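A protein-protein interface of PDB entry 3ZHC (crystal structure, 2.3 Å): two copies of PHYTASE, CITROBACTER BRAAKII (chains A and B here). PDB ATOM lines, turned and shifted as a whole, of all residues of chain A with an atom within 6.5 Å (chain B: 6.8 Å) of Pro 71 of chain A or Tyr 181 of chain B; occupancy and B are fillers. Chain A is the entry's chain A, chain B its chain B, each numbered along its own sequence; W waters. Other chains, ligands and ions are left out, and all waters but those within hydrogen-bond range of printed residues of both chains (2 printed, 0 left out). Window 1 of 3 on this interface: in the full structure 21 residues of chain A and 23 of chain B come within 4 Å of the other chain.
Hydrophobic or aromatic side chains of chain B within 4 Å of the printed part of chain A: Tyr 181. Printed residues of chain A that touch a printed residue of chain B: Pro 71, Arg 72 and Glu 75. Hydrophobic or aromatic side chains of chain A that line the printed part of chain B: Pro 71. Among the printed residues, 4 pairs touch across the chains.
Of chain B, only Arg 180 and Tyr 181 come within 4 Å of Pro 71 of chain A. Tyr 181 of chain B touches one residue of chain A. Printed residues of chain B within 4 Å of Glu 75 of chain A: Arg 180 (3.0 Å). Of the printed residues of chain A, Arg 180 of chain B touches Pro 71, Arg 72 and Glu 75. Of the printed residues of chain B, Arg 72 of chain A touches Arg 180 (3.9 Å). Leu 69 of chain A touches none of the printed residues of chain B. Gly 74 of chain A touches none of the printed residues of chain B. The nearest printed residue of chain B that does not touch Pro 71 of chain A is Ser 269 of chain B (5.6 Å). The nearest printed residue of chain A that does not touch Tyr 181 of chain B is Arg 72 of chain A (6.2 Å).
Water W1 lies within hydrogen-bond range of OD2 of Asp 276 of chain B and OD2 of Asp 63 of chain A. Water W2 lies within hydrogen-bond range of O of Leu 176 of chain B (2.6 Å) and OE2 of Glu 75 of chain A (2.7 Å).
The side-chain carboxylate of Glu 75 of chain A is in salt-bridge range of the guanidinium group of Arg 180 of chain B (3.7 Å).
CG of Arg 180 of chain B touches O of Pro 71 of chain A (3.4 Å). OH of Tyr 181 of chain B touches CG of Pro 71 of chain A (3.4 Å). CA of Arg 72 of chain A touches CD of Arg 180 of chain B, at 3.9 Å.
The backbone carbonyl oxygen (O) of Gln 248 of chain A sits close to the guanidinium group (NH1) of Arg 72 of chain A (3.2 Å).
No position is printed for both chains.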
ATOM      1  N   VAL A  41      -5.395 -14.379  -6.002  1.00  0.00           N
ATOM      2  CA  VAL A  41      -4.387 -13.864  -5.055  1.00  0.00           C
ATOM      3  C   VAL A  41      -2.978 -14.152  -5.597  1.00  0.00           C
ATOM      4  O   VAL A  41      -2.679 -15.269  -6.008  1.00  0.00           O
ATOM      5  CB  VAL A  41      -4.566 -14.438  -3.637  1.00  0.00           C
ATOM      6  CG1 VAL A  41      -3.373 -14.064  -2.717  1.00  0.00           C
ATOM      7  CG2 VAL A  41      -5.888 -13.958  -3.044  1.00  0.00           C
ATOM      8  N   ASP A  63       6.618 -17.210  -1.403  1.00  0.00           N
ATOM      9  CA  ASP A  63       7.324 -18.387  -1.998  1.00  0.00           C
ATOM     10  C   ASP A  63       6.945 -18.685  -3.477  1.00  0.00           C
ATOM     11  O   ASP A  63       7.152 -19.794  -3.960  1.00  0.00           O
ATOM     12  CB  ASP A  63       7.215 -19.641  -1.071  1.00  0.00           C
ATOM     13  CG  ASP A  63       5.811 -20.106  -0.848  1.00  0.00           C
ATOM     14  OD1 ASP A  63       4.937 -19.915  -1.726  1.00  0.00           O
ATOM     15  OD2 ASP A  63       5.568 -20.693   0.231  1.00  0.00           O
ATOM     16  N   VAL A  64       6.389 -17.679  -4.159  1.00  0.00           N
ATOM     17  CA  VAL A  64       6.187 -17.698  -5.608  1.00  0.00           C
ATOM     18  C   VAL A  64       6.806 -16.408  -6.135  1.00  0.00           C
ATOM     19  O   VAL A  64       6.935 -15.444  -5.367  1.00  0.00           O
ATOM     20  CB  VAL A  64       4.706 -17.778  -6.027  1.00  0.00           C
ATOM     21  CG1 VAL A  64       4.072 -19.050  -5.498  1.00  0.00           C
ATOM     22  CG2 VAL A  64       3.917 -16.509  -5.572  1.00  0.00           C
ATOM     23  N   LEU A  69       0.577 -15.910  -9.387  1.00  0.00           N
ATOM     24  CA  LEU A  69      -0.522 -16.451  -8.620  1.00  0.00           C
ATOM     25  C   LEU A  69       0.015 -17.473  -7.621  1.00  0.00           C
ATOM     26  O   LEU A  69       0.915 -18.241  -7.951  1.00  0.00           O
ATOM     27  CB  LEU A  69      -1.526 -17.148  -9.542  1.00  0.00           C
ATOM     28  CG  LEU A  69      -2.968 -17.210  -9.091  1.00  0.00           C
ATOM     29  CD1 LEU A  69      -3.571 -15.858  -9.234  1.00  0.00           C
ATOM     30  CD2 LEU A  69      -3.759 -18.231  -9.920  1.00  0.00           C
ATOM     31  N   THR A  70      -0.530 -17.466  -6.402  1.00  0.00           N
ATOM     32  CA  THR A  70      -0.204 -18.482  -5.417  1.00  0.00           C
ATOM     33  C   THR A  70      -1.141 -19.654  -5.671  1.00  0.00           C
ATOM     34  O   THR A  70      -2.233 -19.459  -6.254  1.00  0.00           O
ATOM     35  CB  THR A  70      -0.382 -18.002  -3.946  1.00  0.00           C
ATOM     36  OG1 THR A  70      -1.753 -17.678  -3.707  1.00  0.00           O
ATOM     37  CG2 THR A  70       0.519 -16.795  -3.634  1.00  0.00           C
ATOM     38  N   PRO A  71      -0.733 -20.882  -5.257  1.00  0.00           N
ATOM     39  CA  PRO A  71      -1.639 -22.059  -5.308  1.00  0.00           C
ATOM     40  C   PRO A  71      -2.977 -21.791  -4.607  1.00  0.00           C
ATOM     41  O   PRO A  71      -4.048 -22.164  -5.122  1.00  0.00           O
ATOM     42  CB  PRO A  71      -0.848 -23.143  -4.575  1.00  0.00           C
ATOM     43  CG  PRO A  71       0.579 -22.774  -4.779  1.00  0.00           C
ATOM     44  CD  PRO A  71       0.640 -21.264  -4.872  1.00  0.00           C
ATOM     45  N   ARG A  72      -2.903 -21.146  -3.450  1.00  0.00           N
ATOM     46  CA  ARG A  72      -4.100 -20.769  -2.694  1.00  0.00           C
ATOM     47  C   ARG A  72      -4.965 -19.764  -3.468  1.00  0.00           C
ATOM     48  O   ARG A  72      -6.193 -19.817  -3.396  1.00  0.00           O
ATOM     49  CB  ARG A  72      -3.702 -20.220  -1.345  1.00  0.00           C
ATOM     50  CG  ARG A  72      -4.819 -19.794  -0.520  1.00  0.00           C
ATOM     51  CD  ARG A  72      -4.442 -19.859   0.896  1.00  0.00           C
ATOM     52  NE  ARG A  72      -5.358 -19.089   1.681  1.00  0.00           N
ATOM     53  CZ  ARG A  72      -5.386 -19.094   2.988  1.00  0.00           C
ATOM     54  NH1 ARG A  72      -4.544 -19.838   3.684  1.00  0.00           N
ATOM     55  NH2 ARG A  72      -6.257 -18.356   3.588  1.00  0.00           N
ATOM     56  N   GLY A  73      -4.319 -18.852  -4.203  1.00  0.00           N
ATOM     57  CA  GLY A  73      -5.033 -17.905  -5.057  1.00  0.00           C
ATOM     58  C   GLY A  73      -5.811 -18.682  -6.113  1.00  0.00           C
ATOM     59  O   GLY A  73      -6.967 -18.382  -6.386  1.00  0.00           O
ATOM     60  N   GLY A  74      -5.151 -19.693  -6.695  1.00  0.00           N
ATOM     61  CA  GLY A  74      -5.778 -20.611  -7.635  1.00  0.00           C
ATOM     62  C   GLY A  74      -6.969 -21.343  -7.035  1.00  0.00           C
ATOM     63  O   GLY A  74      -8.003 -21.460  -7.680  1.00  0.00           O
ATOM     64  N   GLU A  75      -6.828 -21.829  -5.797  1.00  0.00           N
ATOM     65  CA  GLU A  75      -7.943 -22.522  -5.111  1.00  0.00           C
ATOM     66  C   GLU A  75      -9.135 -21.582  -4.916  1.00  0.00           C
ATOM     67  O   GLU A  75     -10.266 -21.974  -5.150  1.00  0.00           O
ATOM     68  CB  GLU A  75      -7.520 -23.104  -3.757  1.00  0.00           C
ATOM     69  CG  GLU A  75      -8.624 -23.979  -3.062  1.00  0.00           C
ATOM     70  CD  GLU A  75      -8.221 -24.480  -1.646  1.00  0.00           C
ATOM     71  OE1 GLU A  75      -7.073 -24.274  -1.238  1.00  0.00           O
ATOM     72  OE2 GLU A  75      -9.078 -25.087  -0.945  1.00  0.00           O
ATOM     73  N   LEU A  76      -8.866 -20.347  -4.490  1.00  0.00           N
ATOM     74  CA  LEU A  76      -9.940 -19.336  -4.280  1.00  0.00           C
ATOM     75  C   LEU A  76     -10.721 -19.040  -5.562  1.00  0.00           C
ATOM     76  O   LEU A  76     -11.951 -18.863  -5.509  1.00  0.00           O
ATOM     77  CB  LEU A  76      -9.376 -18.059  -3.667  1.00  0.00           C
ATOM     78  CG  LEU A  76      -8.981 -18.142  -2.189  1.00  0.00           C
ATOM     79  CD1 LEU A  76      -8.227 -16.886  -1.755  1.00  0.00           C
ATOM     80  CD2 LEU A  76     -10.224 -18.365  -1.304  1.00  0.00           C
ATOM     81  N   GLN A 248      -4.128 -14.374   1.353  1.00  0.00           N
ATOM     82  CA  GLN A 248      -3.203 -15.514   1.247  1.00  0.00           C
ATOM     83  C   GLN A 248      -3.157 -16.372   2.549  1.00  0.00           C
ATOM     84  O   GLN A 248      -2.607 -17.498   2.551  1.00  0.00           O
ATOM     85  CB  GLN A 248      -1.791 -15.004   0.874  1.00  0.00           C
ATOM     86  CG  GLN A 248      -0.664 -16.074   0.711  1.00  0.00           C
ATOM     87  CD  GLN A 248      -0.969 -17.100  -0.354  1.00  0.00           C
ATOM     88  OE1 GLN A 248      -1.784 -16.863  -1.248  1.00  0.00           O
ATOM     89  NE2 GLN A 248      -0.316 -18.252  -0.268  1.00  0.00           N
ATOM     90  N   LEU B 176      -7.796 -32.156  -0.561  1.00  0.00           N
ATOM     91  CA  LEU B 176      -7.925 -30.668  -0.678  1.00  0.00           C
ATOM     92  C   LEU B 176      -6.616 -30.026  -1.164  1.00  0.00           C
ATOM     93  O   LEU B 176      -6.646 -29.059  -1.920  1.00  0.00           O
ATOM     94  CB  LEU B 176      -8.356 -30.008   0.644  1.00  0.00           C
ATOM     95  CG  LEU B 176      -9.772 -30.270   1.182  1.00  0.00           C
ATOM     96  CD1 LEU B 176      -9.965 -29.498   2.488  1.00  0.00           C
ATOM     97  CD2 LEU B 176     -10.870 -29.923   0.179  1.00  0.00           C
ATOM     98  N   TYR B 177      -5.476 -30.568  -0.720  1.00  0.00           N
ATOM     99  CA  TYR B 177      -4.157 -30.111  -1.191  1.00  0.00           C
ATOM    100  C   TYR B 177      -4.008 -30.469  -2.689  1.00  0.00           C
ATOM    101  O   TYR B 177      -3.504 -29.682  -3.459  1.00  0.00           O
ATOM    102  CB  TYR B 177      -3.035 -30.731  -0.351  1.00  0.00           C
ATOM    103  CG  TYR B 177      -1.745 -29.948  -0.277  1.00  0.00           C
ATOM    104  CD1 TYR B 177      -1.710 -28.684   0.332  1.00  0.00           C
ATOM    105  CD2 TYR B 177      -0.545 -30.473  -0.782  1.00  0.00           C
ATOM    106  CE1 TYR B 177      -0.528 -27.951   0.423  1.00  0.00           C
ATOM    107  CE2 TYR B 177       0.665 -29.740  -0.698  1.00  0.00           C
ATOM    108  CZ  TYR B 177       0.657 -28.473  -0.088  1.00  0.00           C
ATOM    109  OH  TYR B 177       1.819 -27.730   0.014  1.00  0.00           O
ATOM    110  N   THR B 178      -4.466 -31.666  -3.078  1.00  0.00           N
ATOM    111  CA  THR B 178      -4.482 -32.076  -4.490  1.00  0.00           C
ATOM    112  C   THR B 178      -5.344 -31.092  -5.331  1.00  0.00           C
ATOM    113  O   THR B 178      -4.885 -30.662  -6.398  1.00  0.00           O
ATOM    114  CB  THR B 178      -4.944 -33.535  -4.659  1.00  0.00           C
ATOM    115  OG1 THR B 178      -4.037 -34.393  -3.949  1.00  0.00           O
ATOM    116  CG2 THR B 178      -4.990 -33.935  -6.138  1.00  0.00           C
ATOM    117  N   GLN B 179      -6.565 -30.736  -4.840  1.00  0.00           N
ATOM    118  CA  GLN B 179      -7.437 -29.748  -5.551  1.00  0.00           C
ATOM    119  C   GLN B 179      -6.731 -28.402  -5.753  1.00  0.00           C
ATOM    120  O   GLN B 179      -6.919 -27.743  -6.778  1.00  0.00           O
ATOM    121  CB  GLN B 179      -8.807 -29.525  -4.863  1.00  0.00           C
ATOM    122  CG  GLN B 179      -9.904 -30.477  -5.348  1.00  0.00           C
ATOM    123  CD  GLN B 179      -9.896 -31.786  -4.631  1.00  0.00           C
ATOM    124  OE1 GLN B 179      -9.601 -32.832  -5.216  1.00  0.00           O
ATOM    125  NE2 GLN B 179     -10.210 -31.749  -3.334  1.00  0.00           N
ATOM    126  N   ARG B 180      -5.925 -28.009  -4.781  1.00  0.00           N
ATOM    127  CA  ARG B 180      -5.168 -26.759  -4.849  1.00  0.00           C
ATOM    128  C   ARG B 180      -4.121 -26.750  -5.987  1.00  0.00           C
ATOM    129  O   ARG B 180      -3.850 -25.701  -6.577  1.00  0.00           O
ATOM    130  CB  ARG B 180      -4.498 -26.498  -3.498  1.00  0.00           C
ATOM    131  CG  ARG B 180      -3.990 -25.092  -3.314  1.00  0.00           C
ATOM    132  CD  ARG B 180      -4.132 -24.624  -1.846  1.00  0.00           C
ATOM    133  NE  ARG B 180      -2.961 -24.759  -1.036  1.00  0.00           N
ATOM    134  CZ  ARG B 180      -2.930 -24.491   0.279  1.00  0.00           C
ATOM    135  NH1 ARG B 180      -4.040 -24.074   0.936  1.00  0.00           N
ATOM    136  NH2 ARG B 180      -1.790 -24.648   0.949  1.00  0.00           N
ATOM    137  N   TYR B 181      -3.546 -27.926  -6.278  1.00  0.00           N
ATOM    138  CA  TYR B 181      -2.538 -28.090  -7.328  1.00  0.00           C
ATOM    139  C   TYR B 181      -3.064 -28.866  -8.572  1.00  0.00           C
ATOM    140  O   TYR B 181      -2.271 -29.453  -9.294  1.00  0.00           O
ATOM    141  CB  TYR B 181      -1.287 -28.770  -6.727  1.00  0.00           C
ATOM    142  CG  TYR B 181      -0.557 -27.911  -5.728  1.00  0.00           C
ATOM    143  CD1 TYR B 181      -0.931 -27.893  -4.377  1.00  0.00           C
ATOM    144  CD2 TYR B 181       0.520 -27.101  -6.120  1.00  0.00           C
ATOM    145  CE1 TYR B 181      -0.249 -27.087  -3.430  1.00  0.00           C
ATOM    146  CE2 TYR B 181       1.204 -26.295  -5.184  1.00  0.00           C
ATOM    147  CZ  TYR B 181       0.806 -26.297  -3.843  1.00  0.00           C
ATOM    148  OH  TYR B 181       1.461 -25.520  -2.936  1.00  0.00           O
ATOM    149  N   GLN B 182      -4.393 -28.852  -8.823  1.00  0.00           N
ATOM    150  CA  GLN B 182      -4.995 -29.581  -9.996  1.00  0.00           C
ATOM    151  C   GLN B 182      -4.300 -29.299 -11.310  1.00  0.00           C
ATOM    152  O   GLN B 182      -3.846 -30.217 -11.972  1.00  0.00           O
ATOM    153  CB  GLN B 182      -6.484 -29.238 -10.196  1.00  0.00           C
ATOM    154  CG  GLN B 182      -7.398 -29.939  -9.291  1.00  0.00           C
ATOM    155  CD  GLN B 182      -8.885 -29.667  -9.595  1.00  0.00           C
ATOM    156  OE1 GLN B 182      -9.638 -29.179  -8.717  1.00  0.00           O
ATOM    157  NE2 GLN B 182      -9.318 -29.976 -10.843  1.00  0.00           N
ATOM    158  N   SER B 183      -4.232 -28.016 -11.673  1.00  0.00           N
ATOM    159  CA  SER B 183      -3.650 -27.586 -12.966  1.00  0.00           C
ATOM    160  C   SER B 183      -2.180 -27.974 -13.120  1.00  0.00           C
ATOM    161  O   SER B 183      -1.736 -28.235 -14.238  1.00  0.00           O
ATOM    162  CB  SER B 183      -3.819 -26.084 -13.161  1.00  0.00           C
ATOM    163  OG  SER B 183      -3.125 -25.376 -12.159  1.00  0.00           O
ATOM    164  N   SER B 184      -1.434 -28.008 -12.004  1.00  0.00           N
ATOM    165  CA  SER B 184      -0.027 -28.472 -12.017  1.00  0.00           C
ATOM    166  C   SER B 184       0.046 -29.946 -12.405  1.00  0.00           C
ATOM    167  O   SER B 184       0.898 -30.337 -13.213  1.00  0.00           O
ATOM    168  CB  SER B 184       0.663 -28.251 -10.660  1.00  0.00           C
ATOM    169  OG  SER B 184       0.992 -26.897 -10.487  1.00  0.00           O
ATOM    170  N   PHE B 185      -0.845 -30.754 -11.823  1.00  0.00           N
ATOM    171  CA  PHE B 185      -0.946 -32.172 -12.173  1.00  0.00           C
ATOM    172  C   PHE B 185      -1.348 -32.364 -13.643  1.00  0.00           C
ATOM    173  O   PHE B 185      -0.864 -33.288 -14.281  1.00  0.00           O
ATOM    174  CB  PHE B 185      -1.918 -32.929 -11.253  1.00  0.00           C
ATOM    175  CG  PHE B 185      -1.340 -33.281  -9.917  1.00  0.00           C
ATOM    176  CD1 PHE B 185      -0.404 -34.325  -9.798  1.00  0.00           C
ATOM    177  CD2 PHE B 185      -1.723 -32.586  -8.756  1.00  0.00           C
ATOM    178  CE1 PHE B 185       0.134 -34.666  -8.547  1.00  0.00           C
ATOM    179  CE2 PHE B 185      -1.183 -32.923  -7.504  1.00  0.00           C
ATOM    180  CZ  PHE B 185      -0.253 -33.966  -7.403  1.00  0.00           C
ATOM    181  N   ARG B 186      -2.225 -31.491 -14.166  1.00  0.00           N
ATOM    182  CA  ARG B 186      -2.585 -31.524 -15.601  1.00  0.00           C
ATOM    183  C   ARG B 186      -1.354 -31.286 -16.478  1.00  0.00           C
ATOM    184  O   ARG B 186      -1.197 -31.941 -17.519  1.00  0.00           O
ATOM    185  CB  ARG B 186      -3.673 -30.476 -15.971  1.00  0.00           C
ATOM    186  CG  ARG B 186      -5.046 -30.606 -15.263  1.00  0.00           C
ATOM    187  CD  ARG B 186      -5.712 -31.977 -15.479  1.00  0.00           C
ATOM    188  NE  ARG B 186      -5.206 -32.960 -14.535  1.00  0.00           N
ATOM    189  CZ  ARG B 186      -5.619 -33.094 -13.255  1.00  0.00           C
ATOM    190  NH1 ARG B 186      -6.572 -32.311 -12.733  1.00  0.00           N
ATOM    191  NH2 ARG B 186      -5.064 -34.034 -12.489  1.00  0.00           N
ATOM    192  N   TRP B 232       1.563 -37.648  -5.288  1.00  0.00           N
ATOM    193  CA  TRP B 232       2.407 -36.584  -4.676  1.00  0.00           C
ATOM    194  C   TRP B 232       3.929 -36.912  -4.648  1.00  0.00           C
ATOM    195  O   TRP B 232       4.727 -36.132  -5.184  1.00  0.00           O
ATOM    196  CB  TRP B 232       1.872 -36.182  -3.275  1.00  0.00           C
ATOM    197  CG  TRP B 232       0.833 -35.157  -3.397  1.00  0.00           C
ATOM    198  CD1 TRP B 232      -0.506 -35.319  -3.279  1.00  0.00           C
ATOM    199  CD2 TRP B 232       1.052 -33.788  -3.697  1.00  0.00           C
ATOM    200  NE1 TRP B 232      -1.148 -34.116  -3.480  1.00  0.00           N
ATOM    201  CE2 TRP B 232      -0.208 -33.159  -3.739  1.00  0.00           C
ATOM    202  CE3 TRP B 232       2.196 -33.023  -3.933  1.00  0.00           C
ATOM    203  CZ2 TRP B 232      -0.357 -31.789  -4.006  1.00  0.00           C
ATOM    204  CZ3 TRP B 232       2.045 -31.656  -4.199  1.00  0.00           C
ATOM    205  CH2 TRP B 232       0.781 -31.062  -4.233  1.00  0.00           C
ATOM    206  N   ASP B 266       4.826 -24.754 -12.908  1.00  0.00           N
ATOM    207  CA  ASP B 266       3.698 -25.706 -12.697  1.00  0.00           C
ATOM    208  C   ASP B 266       4.227 -27.032 -12.239  1.00  0.00           C
ATOM    209  O   ASP B 266       3.723 -27.614 -11.285  1.00  0.00           O
ATOM    210  CB  ASP B 266       2.907 -25.992 -13.996  1.00  0.00           C
ATOM    211  CG  ASP B 266       1.914 -24.924 -14.356  1.00  0.00           C
ATOM    212  OD1 ASP B 266       1.784 -23.906 -13.636  1.00  0.00           O
ATOM    213  OD2 ASP B 266       1.229 -25.121 -15.405  1.00  0.00           O
ATOM    214  N   SER B 269       6.201 -26.809  -8.794  1.00  0.00           N
ATOM    215  CA  SER B 269       5.319 -26.472  -7.658  1.00  0.00           C
ATOM    216  C   SER B 269       4.950 -27.741  -6.877  1.00  0.00           C
ATOM    217  O   SER B 269       4.754 -27.688  -5.672  1.00  0.00           O
ATOM    218  CB  SER B 269       4.049 -25.758  -8.122  1.00  0.00           C
ATOM    219  OG  SER B 269       4.349 -24.454  -8.560  1.00  0.00           O
ATOM    220  N   LEU B 270       4.861 -28.875  -7.593  1.00  0.00           N
ATOM    221  CA  LEU B 270       4.542 -30.165  -6.983  1.00  0.00           C
ATOM    222  C   LEU B 270       5.681 -30.639  -6.083  1.00  0.00           C
ATOM    223  O   LEU B 270       5.442 -31.046  -4.943  1.00  0.00           O
ATOM    224  CB  LEU B 270       4.203 -31.209  -8.069  1.00  0.00           C
ATOM    225  CG  LEU B 270       2.950 -30.853  -8.911  1.00  0.00           C
ATOM    226  CD1 LEU B 270       2.724 -31.836 -10.089  1.00  0.00           C
ATOM    227  CD2 LEU B 270       1.717 -30.775  -8.011  1.00  0.00           C
ATOM    228  N   ASN B 272       8.203 -28.674  -4.883  1.00  0.00           N
ATOM    229  CA  ASN B 272       8.352 -27.665  -3.820  1.00  0.00           C
ATOM    230  C   ASN B 272       7.306 -27.811  -2.736  1.00  0.00           C
ATOM    231  O   ASN B 272       7.622 -27.647  -1.586  1.00  0.00           O
ATOM    232  CB  ASN B 272       8.316 -26.237  -4.391  1.00  0.00           C
ATOM    233  CG  ASN B 272       9.551 -25.897  -5.215  1.00  0.00           C
ATOM    234  OD1 ASN B 272      10.676 -26.287  -4.886  1.00  0.00           O
ATOM    235  ND2 ASN B 272       9.344 -25.155  -6.290  1.00  0.00           N
ATOM    236  N   ALA B 273       6.057 -28.124  -3.130  1.00  0.00           N
ATOM    237  CA  ALA B 273       4.960 -28.361  -2.181  1.00  0.00           C
ATOM    238  C   ALA B 273       5.139 -29.644  -1.389  1.00  0.00           C
ATOM    239  O   ALA B 273       4.773 -29.686  -0.227  1.00  0.00           O
ATOM    240  CB  ALA B 273       3.588 -28.354  -2.902  1.00  0.00           C
ATOM    241  N   GLN B 274       5.697 -30.702  -2.005  1.00  0.00           N
ATOM    242  CA  GLN B 274       5.894 -31.960  -1.253  1.00  0.00           C
ATOM    243  C   GLN B 274       7.015 -31.755  -0.212  1.00  0.00           C
ATOM    244  O   GLN B 274       6.884 -32.221   0.933  1.00  0.00           O
ATOM    245  CB  GLN B 274       6.163 -33.163  -2.143  1.00  0.00           C
ATOM    246  CG  GLN B 274       5.503 -34.423  -1.560  1.00  0.00           C
ATOM    247  CD  GLN B 274       6.393 -35.599  -1.590  1.00  0.00           C
ATOM    248  OE1 GLN B 274       5.995 -36.710  -1.234  1.00  0.00           O
ATOM    249  NE2 GLN B 274       7.633 -35.380  -2.004  1.00  0.00           N
ATOM    250  N   ASP B 276       7.716 -28.873   1.117  1.00  0.00           N
ATOM    251  CA  ASP B 276       7.097 -27.990   2.082  1.00  0.00           C
ATOM    252  C   ASP B 276       6.408 -28.825   3.196  1.00  0.00           C
ATOM    253  O   ASP B 276       6.657 -28.621   4.390  1.00  0.00           O
ATOM    254  CB  ASP B 276       6.107 -27.068   1.395  1.00  0.00           C
ATOM    255  CG  ASP B 276       5.617 -25.941   2.298  1.00  0.00           C
ATOM    256  OD1 ASP B 276       6.216 -25.682   3.374  1.00  0.00           O
ATOM    257  OD2 ASP B 276       4.618 -25.305   1.914  1.00  0.00           O
HETATM  258  O   HOH W   1       4.878 -22.704   2.300  1.00  0.00           O
HETATM  259  O   HOH W   2      -8.820 -27.544  -1.920  1.00  0.00           O
